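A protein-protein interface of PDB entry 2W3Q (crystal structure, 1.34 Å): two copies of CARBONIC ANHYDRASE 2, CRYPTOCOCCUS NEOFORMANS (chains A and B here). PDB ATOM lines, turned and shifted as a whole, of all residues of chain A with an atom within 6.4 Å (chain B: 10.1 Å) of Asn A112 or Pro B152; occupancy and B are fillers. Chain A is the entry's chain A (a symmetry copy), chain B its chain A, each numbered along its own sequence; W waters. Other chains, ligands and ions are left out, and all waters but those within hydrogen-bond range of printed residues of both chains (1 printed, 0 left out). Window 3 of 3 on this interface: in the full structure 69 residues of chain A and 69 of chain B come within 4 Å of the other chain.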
ATOM      1  N   ASP A 105     -11.331  12.096 -13.162  1.00  0.00           N
ATOM      2  CA  ASP A 105     -11.912  13.115 -12.281  1.00  0.00           C
ATOM      3  C   ASP A 105     -13.260  13.600 -12.796  1.00  0.00           C
ATOM      4  O   ASP A 105     -14.156  13.860 -11.994  1.00  0.00           O
ATOM      5  CB  ASP A 105     -10.970  14.307 -12.093  1.00  0.00           C
ATOM      6  CG  ASP A 105      -9.649  14.016 -11.418  1.00  0.00           C
ATOM      7  OD1 ASP A 105      -9.388  12.929 -10.856  1.00  0.00           O
ATOM      8  OD2 ASP A 105      -8.772  14.911 -11.436  1.00  0.00           O
ATOM      9  N   SER A 107     -15.580  11.855 -14.312  1.00  0.00           N
ATOM     10  CA  SER A 107     -16.584  10.857 -13.999  1.00  0.00           C
ATOM     11  C   SER A 107     -16.846  10.830 -12.508  1.00  0.00           C
ATOM     12  O   SER A 107     -18.006  10.724 -12.079  1.00  0.00           O
ATOM     13  CB  SER A 107     -16.138   9.459 -14.445  1.00  0.00           C
ATOM     14  OG  SER A 107     -16.088   9.381 -15.858  1.00  0.00           O
ATOM     15  N   GLN A 108     -15.769  10.941 -11.736  1.00  0.00           N
ATOM     16  CA  GLN A 108     -15.977  11.006 -10.278  1.00  0.00           C
ATOM     17  C   GLN A 108     -16.799  12.221  -9.870  1.00  0.00           C
ATOM     18  O   GLN A 108     -17.671  12.158  -8.987  1.00  0.00           O
ATOM     19  CB  GLN A 108     -14.653  11.016  -9.537  1.00  0.00           C
ATOM     20  CG  GLN A 108     -13.793   9.788  -9.632  1.00  0.00           C
ATOM     21  CD  GLN A 108     -14.338   8.567  -8.942  1.00  0.00           C
ATOM     22  OE1 GLN A 108     -15.413   8.523  -8.357  1.00  0.00           O
ATOM     23  NE2 GLN A 108     -13.597   7.484  -8.967  1.00  0.00           N
ATOM     24  N   ALA A 109     -16.565  13.360 -10.505  1.00  0.00           N
ATOM     25  CA  ALA A 109     -17.348  14.539 -10.211  1.00  0.00           C
ATOM     26  C   ALA A 109     -18.824  14.376 -10.560  1.00  0.00           C
ATOM     27  O   ALA A 109     -19.705  14.807  -9.836  1.00  0.00           O
ATOM     28  CB  ALA A 109     -16.799  15.771 -10.947  1.00  0.00           C
ATOM     29  N   LEU A 110     -19.070  13.744 -11.701  1.00  0.00           N
ATOM     30  CA  LEU A 110     -20.455  13.524 -12.107  1.00  0.00           C
ATOM     31  C   LEU A 110     -21.164  12.635 -11.088  1.00  0.00           C
ATOM     32  O   LEU A 110     -22.295  12.932 -10.732  1.00  0.00           O
ATOM     33  CB  LEU A 110     -20.550  12.933 -13.500  1.00  0.00           C
ATOM     34  CG  LEU A 110     -21.930  12.708 -14.092  1.00  0.00           C
ATOM     35  CD1 LEU A 110     -21.934  12.847 -15.612  1.00  0.00           C
ATOM     36  CD2 LEU A 110     -22.510  11.330 -13.772  1.00  0.00           C
ATOM     37  N   LEU A 111     -20.511  11.546 -10.671  1.00  0.00           N
ATOM     38  CA  LEU A 111     -21.132  10.638  -9.711  1.00  0.00           C
ATOM     39  C   LEU A 111     -21.365  11.348  -8.388  1.00  0.00           C
ATOM     40  O   LEU A 111     -22.414  11.247  -7.759  1.00  0.00           O
ATOM     41  CB  LEU A 111     -20.236   9.429  -9.497  1.00  0.00           C
ATOM     42  CG  LEU A 111     -20.776   8.397  -8.499  1.00  0.00           C
ATOM     43  CD1 LEU A 111     -22.126   7.882  -8.973  1.00  0.00           C
ATOM     44  CD2 LEU A 111     -19.780   7.264  -8.296  1.00  0.00           C
ATOM     45  N   ASN A 112     -20.357  12.113  -7.933  1.00  0.00           N
ATOM     46  CA  ASN A 112     -20.558  12.795  -6.652  1.00  0.00           C
ATOM     47  C   ASN A 112     -21.709  13.788  -6.695  1.00  0.00           C
ATOM     48  O   ASN A 112     -22.525  13.935  -5.799  1.00  0.00           O
ATOM     49  CB  ASN A 112     -19.231  13.478  -6.263  1.00  0.00           C
ATOM     50  CG  ASN A 112     -19.213  13.935  -4.818  1.00  0.00           C
ATOM     51  OD1 ASN A 112     -19.456  15.088  -4.493  1.00  0.00           O
ATOM     52  ND2 ASN A 112     -18.966  12.985  -3.932  1.00  0.00           N
ATOM     53  N   TYR A 113     -21.778  14.537  -7.799  1.00  0.00           N
ATOM     54  CA  TYR A 113     -22.838  15.498  -8.005  1.00  0.00           C
ATOM     55  C   TYR A 113     -24.193  14.818  -8.090  1.00  0.00           C
ATOM     56  O   TYR A 113     -25.159  15.280  -7.519  1.00  0.00           O
ATOM     57  CB  TYR A 113     -22.565  16.251  -9.272  1.00  0.00           C
ATOM     58  CG  TYR A 113     -23.396  17.420  -9.688  1.00  0.00           C
ATOM     59  CD1 TYR A 113     -23.629  18.534  -8.930  1.00  0.00           C
ATOM     60  CD2 TYR A 113     -23.949  17.411 -10.957  1.00  0.00           C
ATOM     61  CE1 TYR A 113     -24.395  19.573  -9.387  1.00  0.00           C
ATOM     62  CE2 TYR A 113     -24.701  18.465 -11.414  1.00  0.00           C
ATOM     63  CZ  TYR A 113     -24.939  19.556 -10.637  1.00  0.00           C
ATOM     64  OH  TYR A 113     -25.681  20.646 -11.053  1.00  0.00           O
ATOM     65  N   ALA A 114     -24.248  13.706  -8.802  1.00  0.00           N
ATOM     66  CA  ALA A 114     -25.517  12.987  -8.917  1.00  0.00           C
ATOM     67  C   ALA A 114     -26.086  12.559  -7.577  1.00  0.00           C
ATOM     68  O   ALA A 114     -27.286  12.661  -7.323  1.00  0.00           O
ATOM     69  CB  ALA A 114     -25.331  11.776  -9.816  1.00  0.00           C
ATOM     70  N   ILE A 115     -25.179  12.024  -6.740  1.00  0.00           N
ATOM     71  CA  ILE A 115     -25.597  11.510  -5.442  1.00  0.00           C
ATOM     72  C   ILE A 115     -25.795  12.617  -4.407  1.00  0.00           C
ATOM     73  O   ILE A 115     -26.782  12.661  -3.671  1.00  0.00           O
ATOM     74  CB  ILE A 115     -24.590  10.440  -4.942  1.00  0.00           C
ATOM     75  CG1 ILE A 115     -24.484   9.268  -5.907  1.00  0.00           C
ATOM     76  CG2 ILE A 115     -24.962   9.952  -3.569  1.00  0.00           C
ATOM     77  CD1 ILE A 115     -25.808   8.558  -6.072  1.00  0.00           C
ATOM     78  N   MET A 116     -24.830  13.519  -4.327  1.00  0.00           N
ATOM     79  CA  MET A 116     -24.861  14.488  -3.237  1.00  0.00           C
ATOM     80  C   MET A 116     -25.759  15.679  -3.550  1.00  0.00           C
ATOM     81  O   MET A 116     -26.324  16.220  -2.574  1.00  0.00           O
ATOM     82  CB  MET A 116     -23.451  14.934  -2.907  1.00  0.00           C
ATOM     83  CG  MET A 116     -22.475  13.822  -2.590  1.00  0.00           C
ATOM     84  SD  MET A 116     -23.038  12.801  -1.219  1.00  0.00           S
ATOM     85  CE  MET A 116     -22.501  11.201  -1.806  1.00  0.00           C
ATOM     86  N   ASN A 117     -25.908  16.081  -4.825  1.00  0.00           N
ATOM     87  CA  ASN A 117     -26.697  17.266  -5.161  1.00  0.00           C
ATOM     88  C   ASN A 117     -27.978  16.984  -5.937  1.00  0.00           C
ATOM     89  O   ASN A 117     -29.052  17.488  -5.570  1.00  0.00           O
ATOM     90  CB  ASN A 117     -25.789  18.237  -5.925  1.00  0.00           C
ATOM     91  CG  ASN A 117     -24.567  18.587  -5.107  1.00  0.00           C
ATOM     92  OD1 ASN A 117     -23.464  18.250  -5.531  1.00  0.00           O
ATOM     93  ND2 ASN A 117     -24.690  19.225  -3.952  1.00  0.00           N
ATOM     94  N   VAL A 118     -27.885  16.170  -7.008  1.00  0.00           N
ATOM     95  CA  VAL A 118     -29.072  15.889  -7.834  1.00  0.00           C
ATOM     96  C   VAL A 118     -30.083  15.044  -7.058  1.00  0.00           C
ATOM     97  O   VAL A 118     -31.288  15.275  -7.136  1.00  0.00           O
ATOM     98  CB  VAL A 118     -28.689  15.255  -9.163  1.00  0.00           C
ATOM     99  CG1 VAL A 118     -29.926  14.973  -9.982  1.00  0.00           C
ATOM    100  CG2 VAL A 118     -27.739  16.146  -9.981  1.00  0.00           C
ATOM    101  N   PRO A 192     -15.071   6.893  -3.921  1.00  0.00           N
ATOM    102  CA  PRO A 192     -15.274   7.601  -2.628  1.00  0.00           C
ATOM    103  C   PRO A 192     -16.706   8.057  -2.422  1.00  0.00           C
ATOM    104  O   PRO A 192     -17.192   8.036  -1.300  1.00  0.00           O
ATOM    105  CB  PRO A 192     -14.300   8.772  -2.750  1.00  0.00           C
ATOM    106  CG  PRO A 192     -13.231   8.293  -3.705  1.00  0.00           C
ATOM    107  CD  PRO A 192     -13.981   7.479  -4.731  1.00  0.00           C
ATOM    108  N   THR A 193     -17.398   8.426  -3.495  1.00  0.00           N
ATOM    109  CA  THR A 193     -18.802   8.866  -3.376  1.00  0.00           C
ATOM    110  C   THR A 193     -19.700   7.781  -2.787  1.00  0.00           C
ATOM    111  O   THR A 193     -20.451   8.001  -1.849  1.00  0.00           O
ATOM    112  CB  THR A 193     -19.359   9.300  -4.755  1.00  0.00           C
ATOM    113  OG1 THR A 193     -18.664  10.481  -5.216  1.00  0.00           O
ATOM    114  CG2 THR A 193     -20.838   9.643  -4.639  1.00  0.00           C
ATOM    115  N   VAL B  96     -21.185  16.595 -16.978  1.00  0.00           N
ATOM    116  CA  VAL B  96     -21.756  17.733 -16.270  1.00  0.00           C
ATOM    117  C   VAL B  96     -21.362  19.022 -16.987  1.00  0.00           C
ATOM    118  O   VAL B  96     -20.201  19.348 -17.215  1.00  0.00           O
ATOM    119  CB  VAL B  96     -21.319  17.746 -14.797  1.00  0.00           C
ATOM    120  CG1 VAL B  96     -21.741  19.067 -14.138  1.00  0.00           C
ATOM    121  CG2 VAL B  96     -21.865  16.510 -14.096  1.00  0.00           C
ATOM    122  N   GLN B  99     -18.893  20.021 -20.921  1.00  0.00           N
ATOM    123  CA  GLN B  99     -17.502  20.431 -21.112  1.00  0.00           C
ATOM    124  C   GLN B  99     -16.799  19.412 -22.017  1.00  0.00           C
ATOM    125  O   GLN B  99     -17.020  18.198 -21.968  1.00  0.00           O
ATOM    126  CB  GLN B  99     -16.725  20.591 -19.801  1.00  0.00           C
ATOM    127  CG  GLN B  99     -17.210  21.728 -18.899  1.00  0.00           C
ATOM    128  CD  GLN B  99     -16.288  22.027 -17.752  1.00  0.00           C
ATOM    129  OE1 GLN B  99     -15.272  22.669 -17.951  1.00  0.00           O
ATOM    130  NE2 GLN B  99     -16.633  21.577 -16.528  1.00  0.00           N
ATOM    131  N   LYS B 101     -13.007  19.032 -22.111  1.00  0.00           N
ATOM    132  CA  LYS B 101     -11.752  19.461 -21.512  1.00  0.00           C
ATOM    133  C   LYS B 101     -10.576  18.903 -22.325  1.00  0.00           C
ATOM    134  O   LYS B 101     -10.483  17.688 -22.521  1.00  0.00           O
ATOM    135  CB  LYS B 101     -11.663  18.974 -20.065  1.00  0.00           C
ATOM    136  CG  LYS B 101     -12.764  19.537 -19.147  1.00  0.00           C
ATOM    137  CD  LYS B 101     -12.432  19.223 -17.711  1.00  0.00           C
ATOM    138  CE  LYS B 101     -13.389  19.919 -16.767  1.00  0.00           C
ATOM    139  NZ  LYS B 101     -12.958  19.962 -15.381  1.00  0.00           N
ATOM    140  N   ALA B 136     -24.148  27.029 -10.636  1.00  0.00           N
ATOM    141  CA  ALA B 136     -23.223  26.970  -9.493  1.00  0.00           C
ATOM    142  C   ALA B 136     -21.989  27.801  -9.763  1.00  0.00           C
ATOM    143  O   ALA B 136     -21.466  28.520  -8.916  1.00  0.00           O
ATOM    144  CB  ALA B 136     -22.905  25.504  -9.215  1.00  0.00           C
ATOM    145  N   GLY B 149     -10.411  24.981  -4.798  1.00  0.00           N
ATOM    146  CA  GLY B 149     -11.618  24.213  -4.862  1.00  0.00           C
ATOM    147  C   GLY B 149     -12.055  23.210  -3.836  1.00  0.00           C
ATOM    148  O   GLY B 149     -11.520  22.114  -3.610  1.00  0.00           O
ATOM    149  N   GLY B 150     -13.166  23.493  -3.134  1.00  0.00           N
ATOM    150  CA  GLY B 150     -13.649  22.718  -2.022  1.00  0.00           C
ATOM    151  C   GLY B 150     -14.493  21.503  -2.217  1.00  0.00           C
ATOM    152  O   GLY B 150     -14.628  20.715  -1.253  1.00  0.00           O
ATOM    153  N   THR B 151     -15.088  21.240  -3.362  1.00  0.00           N
ATOM    154  CA  THR B 151     -15.809  19.982  -3.576  1.00  0.00           C
ATOM    155  C   THR B 151     -15.346  19.405  -4.903  1.00  0.00           C
ATOM    156  O   THR B 151     -14.805  20.214  -5.657  1.00  0.00           O
ATOM    157  CB  THR B 151     -17.339  20.159  -3.704  1.00  0.00           C
ATOM    158  OG1 THR B 151     -17.585  21.190  -4.669  1.00  0.00           O
ATOM    159  CG2 THR B 151     -18.020  20.644  -2.441  1.00  0.00           C
ATOM    160  N   PRO B 152     -15.608  18.144  -5.212  1.00  0.00           N
ATOM    161  CA  PRO B 152     -15.297  17.649  -6.567  1.00  0.00           C
ATOM    162  C   PRO B 152     -15.970  18.534  -7.611  1.00  0.00           C
ATOM    163  O   PRO B 152     -15.346  18.824  -8.629  1.00  0.00           O
ATOM    164  CB  PRO B 152     -15.875  16.247  -6.595  1.00  0.00           C
ATOM    165  CG  PRO B 152     -15.814  15.856  -5.139  1.00  0.00           C
ATOM    166  CD  PRO B 152     -16.197  17.092  -4.387  1.00  0.00           C
ATOM    167  N   LEU B 153     -17.216  18.921  -7.364  1.00  0.00           N
ATOM    168  CA  LEU B 153     -17.921  19.702  -8.352  1.00  0.00           C
ATOM    169  C   LEU B 153     -17.196  21.015  -8.614  1.00  0.00           C
ATOM    170  O   LEU B 153     -16.954  21.391  -9.770  1.00  0.00           O
ATOM    171  CB  LEU B 153     -19.356  19.924  -7.862  1.00  0.00           C
ATOM    172  CG  LEU B 153     -20.175  20.832  -8.780  1.00  0.00           C
ATOM    173  CD1 LEU B 153     -20.396  20.127 -10.092  1.00  0.00           C
ATOM    174  CD2 LEU B 153     -21.473  21.254  -8.103  1.00  0.00           C
ATOM    175  N   VAL B 154     -16.869  21.745  -7.550  1.00  0.00           N
ATOM    176  CA  VAL B 154     -16.275  23.067  -7.766  1.00  0.00           C
ATOM    177  C   VAL B 154     -14.958  22.936  -8.483  1.00  0.00           C
ATOM    178  O   VAL B 154     -14.574  23.728  -9.346  1.00  0.00           O
ATOM    179  CB  VAL B 154     -16.117  23.859  -6.444  1.00  0.00           C
ATOM    180  CG1 VAL B 154     -15.319  25.146  -6.608  1.00  0.00           C
ATOM    181  CG2 VAL B 154     -17.495  24.250  -5.895  1.00  0.00           C
ATOM    182  N   ARG B 155     -14.191  21.908  -8.136  1.00  0.00           N
ATOM    183  CA  ARG B 155     -12.927  21.738  -8.857  1.00  0.00           C
ATOM    184  C   ARG B 155     -13.176  21.450 -10.329  1.00  0.00           C
ATOM    185  O   ARG B 155     -12.530  21.978 -11.252  1.00  0.00           O
ATOM    186  CB  ARG B 155     -12.130  20.624  -8.179  1.00  0.00           C
ATOM    187  CG  ARG B 155     -11.811  20.974  -6.724  1.00  0.00           C
ATOM    188  CD  ARG B 155     -10.794  20.081  -6.053  1.00  0.00           C
ATOM    189  NE  ARG B 155     -11.378  18.830  -5.586  1.00  0.00           N
ATOM    190  CZ  ARG B 155     -11.992  18.631  -4.432  1.00  0.00           C
ATOM    191  NH1 ARG B 155     -12.161  19.578  -3.517  1.00  0.00           N
ATOM    192  NH2 ARG B 155     -12.461  17.417  -4.177  1.00  0.00           N
ATOM    193  N   TYR B 156     -14.174  20.602 -10.564  1.00  0.00           N
ATOM    194  CA  TYR B 156     -14.550  20.235 -11.930  1.00  0.00           C
ATOM    195  C   TYR B 156     -15.006  21.427 -12.746  1.00  0.00           C
ATOM    196  O   TYR B 156     -14.831  21.524 -13.976  1.00  0.00           O
ATOM    197  CB  TYR B 156     -15.671  19.201 -11.867  1.00  0.00           C
ATOM    198  CG  TYR B 156     -16.288  18.882 -13.212  1.00  0.00           C
ATOM    199  CD1 TYR B 156     -15.659  18.011 -14.085  1.00  0.00           C
ATOM    200  CD2 TYR B 156     -17.476  19.448 -13.622  1.00  0.00           C
ATOM    201  CE1 TYR B 156     -16.221  17.716 -15.315  1.00  0.00           C
ATOM    202  CE2 TYR B 156     -18.049  19.174 -14.835  1.00  0.00           C
ATOM    203  CZ  TYR B 156     -17.400  18.299 -15.681  1.00  0.00           C
ATOM    204  OH  TYR B 156     -17.951  18.018 -16.903  1.00  0.00           O
ATOM    205  N   LEU B 157     -15.671  22.344 -12.067  1.00  0.00           N
ATOM    206  CA  LEU B 157     -16.222  23.493 -12.769  1.00  0.00           C
ATOM    207  C   LEU B 157     -15.221  24.633 -12.960  1.00  0.00           C
ATOM    208  O   LEU B 157     -15.607  25.690 -13.480  1.00  0.00           O
ATOM    209  CB  LEU B 157     -17.426  24.049 -11.966  1.00  0.00           C
ATOM    210  CG  LEU B 157     -18.678  23.178 -11.834  1.00  0.00           C
ATOM    211  CD1 LEU B 157     -19.715  23.778 -10.890  1.00  0.00           C
ATOM    212  CD2 LEU B 157     -19.276  22.972 -13.209  1.00  0.00           C
ATOM    213  N   GLU B 158     -13.985  24.466 -12.517  1.00  0.00           N
ATOM    214  CA  GLU B 158     -12.998  25.544 -12.609  1.00  0.00           C
ATOM    215  C   GLU B 158     -12.955  26.272 -13.931  1.00  0.00           C
ATOM    216  O   GLU B 158     -12.915  27.503 -13.925  1.00  0.00           O
ATOM    217  CB  GLU B 158     -11.591  24.963 -12.289  1.00  0.00           C
ATOM    218  CG  GLU B 158     -10.517  26.007 -12.247  1.00  0.00           C
ATOM    219  CD  GLU B 158      -9.689  26.285 -13.457  1.00  0.00           C
ATOM    220  OE1 GLU B 158     -10.000  25.854 -14.589  1.00  0.00           O
ATOM    221  OE2 GLU B 158      -8.683  27.012 -13.239  1.00  0.00           O
ATOM    222  N   PRO B 159     -12.993  25.586 -15.076  1.00  0.00           N
ATOM    223  CA  PRO B 159     -12.972  26.347 -16.342  1.00  0.00           C
ATOM    224  C   PRO B 159     -14.205  27.220 -16.563  1.00  0.00           C
ATOM    225  O   PRO B 159     -14.087  28.290 -17.186  1.00  0.00           O
ATOM    226  CB  PRO B 159     -12.833  25.276 -17.414  1.00  0.00           C
ATOM    227  CG  PRO B 159     -12.336  24.049 -16.686  1.00  0.00           C
ATOM    228  CD  PRO B 159     -12.970  24.129 -15.317  1.00  0.00           C
ATOM    229  N   ILE B 161     -15.991  28.566 -14.058  1.00  0.00           N
ATOM    230  CA  ILE B 161     -15.804  29.668 -13.100  1.00  0.00           C
ATOM    231  C   ILE B 161     -14.865  30.728 -13.654  1.00  0.00           C
ATOM    232  O   ILE B 161     -15.145  31.938 -13.597  1.00  0.00           O
ATOM    233  CB  ILE B 161     -15.343  29.112 -11.750  1.00  0.00           C
ATOM    234  CG1 ILE B 161     -16.372  28.149 -11.165  1.00  0.00           C
ATOM    235  CG2 ILE B 161     -15.045  30.260 -10.784  1.00  0.00           C
ATOM    236  CD1 ILE B 161     -15.812  27.299 -10.022  1.00  0.00           C
HETATM  237  O   HOH W   1     -19.176  17.715  -5.592  1.00  0.00           O
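No position is printed for both chains.
The backbone carbonyl oxygen of Val B96 sits at hydrogen-bond distance from the side-chain hydroxyl of Tyr B156 (2.6 Å). O of Tyr B156 is in hydrogen-bond range of NE2 of Gln B99 (3.1 Å). The backbone carbonyl oxygen (O) of Tyr B156 is in hydrogen-bond range of the side-chain amino group (NZ) of Lys B101, 2.8 Å away. OG1 of Thr A193 is in hydrogen-bond range of ND2 of Asn A112, 2.8 Å away. O of Tyr A113 sits at hydrogen-bond distance from N of Val A118.
Asn A112 touches just one residue of chain B: Pro B152 (3.8 Å). Pro B152 touches just one residue of chain A: Asn A112. Of the printed residues of chain B, Ala A109 touches Tyr B156. Leu A111 touches none of the printed residues of chain B. No residue of chain B comes within 4 Å of Ala A114. Thr A193 touches none of the printed residues of chain B. Printed residues of chain A within 4 Å of Tyr B156: Ala A109. Of the printed residues of chain A, Leu B153 touches Tyr A113 (3.6 Å). Printed residues of chain A within 4 Å of Val B96: Leu A110 and Tyr A113. Printed residues of chain B within 4 Å of Tyr A113: Val B96 (3.9 Å) and Leu B153 (3.6 Å). Thr B151 touches none of the printed residues of chain A. Leu B157 touches none of the printed residues of chain A. The nearest residue of chain B that does not touch Asn A112 is Leu B153 (5.3 Å). The nearest residue of chain A that does not touch Pro B152 is Ala A109 (4.1 Å).
Printed residues of chain B that touch a printed residue of chain A: Val B96, Pro B152, Leu B153 and Tyr B156. Hydrophobic or aromatic side chains of chain B that line the printed part of chain A: Val B96, Pro B152, Leu B153 and Tyr B156. Printed residues of chain A that touch a printed residue of chain B: Ala A109, Leu A110, Asn A112 and Tyr A113. Among the printed residues, 5 pairs touch across the chains.
Water W1 bridges OD1 of Asn A112 (2.9 Å) and N of Leu B153 (2.9 Å).
Ala A109 touches Tyr B156 (CB to CB, 3.7 Å). CG2 of Val B96 touches CG of Leu A110, at 3.8 Å. CG of Pro B152 touches OD1 of Asn A112, at 3.8 Å. Val B96 touches Tyr A113. Leu B153 touches Tyr A113.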
